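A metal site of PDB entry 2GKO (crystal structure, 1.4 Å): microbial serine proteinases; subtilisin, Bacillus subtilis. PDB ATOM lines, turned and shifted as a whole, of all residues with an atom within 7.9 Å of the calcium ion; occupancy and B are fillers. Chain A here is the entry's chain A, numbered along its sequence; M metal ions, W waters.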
ATOM      1  N   ALA A  26      -6.862   1.480  19.835  1.00  0.00           N
ATOM      2  CA  ALA A  26      -6.542   0.061  19.739  1.00  0.00           C
ATOM      3  C   ALA A  26      -5.153  -0.180  19.172  1.00  0.00           C
ATOM      4  O   ALA A  26      -4.759   0.394  18.176  1.00  0.00           O
ATOM      5  CB  ALA A  26      -7.585  -0.662  18.893  1.00  0.00           C
ATOM      6  N   GLY A  27      -4.412  -1.051  19.846  1.00  0.00           N
ATOM      7  CA  GLY A  27      -3.091  -1.436  19.396  1.00  0.00           C
ATOM      8  C   GLY A  27      -1.950  -0.543  19.838  1.00  0.00           C
ATOM      9  O   GLY A  27      -0.801  -0.959  19.741  1.00  0.00           O
ATOM     10  N   ILE A  28      -2.263   0.657  20.342  1.00  0.00           N
ATOM     11  CA  ILE A  28      -1.219   1.592  20.730  1.00  0.00           C
ATOM     12  C   ILE A  28      -0.977   1.461  22.205  1.00  0.00           C
ATOM     13  O   ILE A  28      -1.916   1.357  22.996  1.00  0.00           O
ATOM     14  CB  ILE A  28      -1.608   3.031  20.381  1.00  0.00           C
ATOM     15  CG1 ILE A  28      -2.040   3.144  18.903  1.00  0.00           C
ATOM     16  CG2 ILE A  28      -0.457   3.978  20.694  1.00  0.00           C
ATOM     17  CD1 ILE A  28      -1.000   2.723  17.907  1.00  0.00           C
ATOM     18  N   ASN A  29       0.298   1.491  22.596  1.00  0.00           N
ATOM     19  CA  ASN A  29       0.683   1.324  23.994  1.00  0.00           C
ATOM     20  C   ASN A  29       1.022   2.670  24.593  1.00  0.00           C
ATOM     21  O   ASN A  29       1.787   3.422  24.008  1.00  0.00           O
ATOM     22  CB  ASN A  29       1.904   0.405  24.097  1.00  0.00           C
ATOM     23  CG  ASN A  29       1.717  -0.875  23.317  1.00  0.00           C
ATOM     24  OD1 ASN A  29       0.973  -1.759  23.770  1.00  0.00           O
ATOM     25  ND2 ASN A  29       2.298  -0.952  22.116  1.00  0.00           N
ATOM     26  N   ILE A  30       0.364   3.015  25.699  1.00  0.00           N
ATOM     27  CA  ILE A  30       0.695   4.202  26.453  1.00  0.00           C
ATOM     28  C   ILE A  30       1.476   3.773  27.687  1.00  0.00           C
ATOM     29  O   ILE A  30       0.975   3.085  28.585  1.00  0.00           O
ATOM     30  CB  ILE A  30      -0.567   5.033  26.845  1.00  0.00           C
ATOM     31  CG1 ILE A  30      -1.360   5.426  25.586  1.00  0.00           C
ATOM     32  CG2 ILE A  30      -0.152   6.288  27.598  1.00  0.00           C
ATOM     33  CD1 ILE A  30      -2.657   6.172  25.866  1.00  0.00           C
ATOM     34  N   ASN A  47      -7.199  -2.865  30.457  1.00  0.00           N
ATOM     35  CA  ASN A  47      -6.201  -2.300  29.559  1.00  0.00           C
ATOM     36  C   ASN A  47      -4.772  -2.558  30.013  1.00  0.00           C
ATOM     37  O   ASN A  47      -3.835  -2.227  29.294  1.00  0.00           O
ATOM     38  CB  ASN A  47      -6.432  -0.810  29.342  1.00  0.00           C
ATOM     39  CG  ASN A  47      -7.561  -0.546  28.378  1.00  0.00           C
ATOM     40  OD1 ASN A  47      -7.846  -1.384  27.526  1.00  0.00           O
ATOM     41  ND2 ASN A  47      -8.193   0.618  28.489  1.00  0.00           N
ATOM     42  N   GLU A  49      -1.394  -4.087  30.260  1.00  0.00           N
ATOM     43  CA  GLU A  49      -0.583  -5.004  29.481  1.00  0.00           C
ATOM     44  C   GLU A  49       0.782  -5.271  30.122  1.00  0.00           C
ATOM     45  O   GLU A  49       1.194  -6.423  30.229  1.00  0.00           O
ATOM     46  CB  GLU A  49      -0.415  -4.478  28.063  1.00  0.00           C
ATOM     47  CG  GLU A  49       0.164  -5.511  27.120  1.00  0.00           C
ATOM     48  CD  GLU A  49       0.015  -5.025  25.708  1.00  0.00           C
ATOM     49  OE1 GLU A  49       0.803  -4.195  25.310  1.00  0.00           O
ATOM     50  OE2 GLU A  49      -0.940  -5.440  24.999  1.00  0.00           O
ATOM     51  N   GLN A  50       1.477  -4.196  30.510  1.00  0.00           N
ATOM     52  CA  GLN A  50       2.757  -4.272  31.205  1.00  0.00           C
ATOM     53  C   GLN A  50       2.685  -3.571  32.542  1.00  0.00           C
ATOM     54  O   GLN A  50       1.910  -2.625  32.721  1.00  0.00           O
ATOM     55  CB  GLN A  50       3.885  -3.674  30.363  1.00  0.00           C
ATOM     56  CG  GLN A  50       4.095  -4.442  29.052  1.00  0.00           C
ATOM     57  CD  GLN A  50       5.440  -4.186  28.394  1.00  0.00           C
ATOM     58  OE1 GLN A  50       5.667  -4.628  27.244  1.00  0.00           O
ATOM     59  NE2 GLN A  50       6.306  -3.467  29.068  1.00  0.00           N
ATOM     60  N   GLU A  95      -9.314   2.092  24.393  1.00  0.00           N
ATOM     61  CA  GLU A  95      -8.855   0.827  23.788  1.00  0.00           C
ATOM     62  C   GLU A  95      -7.335   0.701  23.742  1.00  0.00           C
ATOM     63  O   GLU A  95      -6.821  -0.315  23.300  1.00  0.00           O
ATOM     64  CB  GLU A  95      -9.374   0.712  22.380  1.00  0.00           C
ATOM     65  CG  GLU A  95     -10.895   0.675  22.332  1.00  0.00           C
ATOM     66  CD  GLU A  95     -11.408   0.714  20.905  1.00  0.00           C
ATOM     67  OE1 GLU A  95     -10.946  -0.078  20.082  1.00  0.00           O
ATOM     68  OE2 GLU A  95     -12.286   1.554  20.623  1.00  0.00           O
ATOM     69  N   ALA A  96      -6.622   1.737  24.184  1.00  0.00           N
ATOM     70  CA  ALA A  96      -5.170   1.638  24.271  1.00  0.00           C
ATOM     71  C   ALA A  96      -4.690   0.607  25.315  1.00  0.00           C
ATOM     72  O   ALA A  96      -5.432   0.192  26.220  1.00  0.00           O
ATOM     73  CB  ALA A  96      -4.554   3.005  24.531  1.00  0.00           C
ATOM     74  N   ASP A  97      -3.438   0.189  25.169  1.00  0.00           N
ATOM     75  CA  ASP A  97      -2.828  -0.767  26.081  1.00  0.00           C
ATOM     76  C   ASP A  97      -1.999   0.025  27.073  1.00  0.00           C
ATOM     77  O   ASP A  97      -1.177   0.840  26.669  1.00  0.00           O
ATOM     78  CB  ASP A  97      -1.899  -1.697  25.332  1.00  0.00           C
ATOM     79  CG  ASP A  97      -2.566  -2.505  24.238  1.00  0.00           C
ATOM     80  OD1 ASP A  97      -3.810  -2.633  24.225  1.00  0.00           O
ATOM     81  OD2 ASP A  97      -1.884  -3.083  23.361  1.00  0.00           O
ATOM     82  N   LEU A  98      -2.177  -0.238  28.351  1.00  0.00           N
ATOM     83  CA  LEU A  98      -1.413   0.447  29.399  1.00  0.00           C
ATOM     84  C   LEU A  98      -0.134  -0.303  29.736  1.00  0.00           C
ATOM     85  O   LEU A  98      -0.173  -1.485  30.061  1.00  0.00           O
ATOM     86  CB  LEU A  98      -2.259   0.601  30.671  1.00  0.00           C
ATOM     87  CG  LEU A  98      -1.581   1.189  31.901  1.00  0.00           C
ATOM     88  CD1 LEU A  98      -1.062   2.614  31.603  1.00  0.00           C
ATOM     89  CD2 LEU A  98      -2.547   1.142  33.051  1.00  0.00           C
ATOM     90  N   TRP A  99       0.994   0.412  29.675  1.00  0.00           N
ATOM     91  CA  TRP A  99       2.266  -0.054  30.225  1.00  0.00           C
ATOM     92  C   TRP A  99       2.549   0.817  31.422  1.00  0.00           C
ATOM     93  O   TRP A  99       2.907   1.997  31.280  1.00  0.00           O
ATOM     94  CB  TRP A  99       3.405   0.091  29.219  1.00  0.00           C
ATOM     95  CG  TRP A  99       3.298  -0.759  28.024  1.00  0.00           C
ATOM     96  CD1 TRP A  99       2.234  -1.560  27.647  1.00  0.00           C
ATOM     97  CD2 TRP A  99       4.268  -0.899  26.984  1.00  0.00           C
ATOM     98  NE1 TRP A  99       2.510  -2.189  26.461  1.00  0.00           N
ATOM     99  CE2 TRP A  99       3.751  -1.788  26.023  1.00  0.00           C
ATOM    100  CE3 TRP A  99       5.536  -0.343  26.777  1.00  0.00           C
ATOM    101  CZ2 TRP A  99       4.460  -2.146  24.870  1.00  0.00           C
ATOM    102  CZ3 TRP A  99       6.238  -0.701  25.630  1.00  0.00           C
ATOM    103  CH2 TRP A  99       5.709  -1.602  24.703  1.00  0.00           C
ATOM    104  N   LEU A 129       9.108  -5.622  20.121  1.00  0.00           N
ATOM    105  CA  LEU A 129       7.735  -6.055  19.833  1.00  0.00           C
ATOM    106  C   LEU A 129       7.229  -5.519  18.511  1.00  0.00           C
ATOM    107  O   LEU A 129       6.128  -5.849  18.083  1.00  0.00           O
ATOM    108  CB  LEU A 129       6.808  -5.595  20.957  1.00  0.00           C
ATOM    109  CG  LEU A 129       7.197  -6.060  22.369  1.00  0.00           C
ATOM    110  CD1 LEU A 129       6.112  -5.676  23.394  1.00  0.00           C
ATOM    111  CD2 LEU A 129       7.482  -7.543  22.434  1.00  0.00           C
ATOM    112  N   THR A 131       6.142  -2.471  17.947  1.00  0.00           N
ATOM    113  CA  THR A 131       4.864  -1.895  18.356  1.00  0.00           C
ATOM    114  C   THR A 131       5.041  -0.404  18.621  1.00  0.00           C
ATOM    115  O   THR A 131       6.164   0.074  18.786  1.00  0.00           O
ATOM    116  CB  THR A 131       4.336  -2.648  19.609  1.00  0.00           C
ATOM    117  OG1 THR A 131       2.950  -2.357  19.810  1.00  0.00           O
ATOM    118  CG2 THR A 131       5.045  -2.202  20.871  1.00  0.00           C
ATOM    119  N   LYS A 132       3.922   0.313  18.621  1.00  0.00           N
ATOM    120  CA  LYS A 132       3.927   1.763  18.782  1.00  0.00           C
ATOM    121  C   LYS A 132       3.713   2.107  20.245  1.00  0.00           C
ATOM    122  O   LYS A 132       2.862   1.521  20.932  1.00  0.00           O
ATOM    123  CB  LYS A 132       2.849   2.389  17.879  1.00  0.00           C
ATOM    124  CG  LYS A 132       3.055   2.111  16.387  1.00  0.00           C
ATOM    125  CD  LYS A 132       4.469   2.467  15.922  1.00  0.00           C
ATOM    126  CE  LYS A 132       4.505   2.697  14.422  1.00  0.00           C
ATOM    127  NZ  LYS A 132       5.835   3.139  13.945  1.00  0.00           N
ATOM    128  N   VAL A 133       4.542   3.038  20.723  1.00  0.00           N
ATOM    129  CA  VAL A 133       4.550   3.402  22.134  1.00  0.00           C
ATOM    130  C   VAL A 133       4.478   4.931  22.247  1.00  0.00           C
ATOM    131  O   VAL A 133       5.246   5.671  21.590  1.00  0.00           O
ATOM    132  CB  VAL A 133       5.806   2.860  22.839  1.00  0.00           C
ATOM    133  CG1 VAL A 133       5.815   3.280  24.291  1.00  0.00           C
ATOM    134  CG2 VAL A 133       5.872   1.341  22.733  1.00  0.00           C
HETATM  135 CA    CA M   1       0.173  -3.716  23.210  1.00  0.00          CA
HETATM  136  O   HOH W   1       2.361  -4.393  22.801  1.00  0.00           O
HETATM  137  O   HOH W   2      -0.376  -5.818  22.478  1.00  0.00           O
HETATM  138  O   HOH W   3       0.127  -3.181  21.105  1.00  0.00           O
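The backbone NH of Asp 97 lies within hydrogen-bond range of the backbone carbonyl oxygen of Ile 28 (2.9 Å).
N of Ile 30 is in hydrogen-bond range of O of Asp 97.
The side-chain amide oxygen (OD1) of Asn 29 lies close to the indole nitrogen (NE1) of Trp 99.
ND2 of Asn 29 sits at hydrogen-bond distance from OG1 of Thr 131, at 2.8 Å.
The backbone carbonyl oxygen (O) of Lys 132 is in hydrogen-bond range of the side-chain amide nitrogen (ND2) of Asn 29.
OE1 of Glu 49 sits close to NE1 of Trp 99, at 2.9 Å.
The backbone carbonyl oxygen of Leu 98 is in hydrogen-bond range of the backbone NH of Glu 49.
Within 4 Å of the calcium ion: Asn 29, Glu 49 and Asp 97.
The nearest printed residue that does not touch the calcium ion is Trp 99 (4.3 Å).
The calcium ion is bound by OD2 of Asp 97 (2.2 Å), water W3 (2.2 Å), OD1 of Asn 29 (2.2 Å), OE1 of Glu 49 (2.2 Å), water W2 (2.3 Å), water W1 (2.3 Å) and OE2 of Glu 49 (2.7 Å).
Water W3 lies within hydrogen-bond range of O of Gly 27 (2.8 Å), OG1 of Thr 131 (3.2 Å) and ND2 of Asn 29 (3.3 Å).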
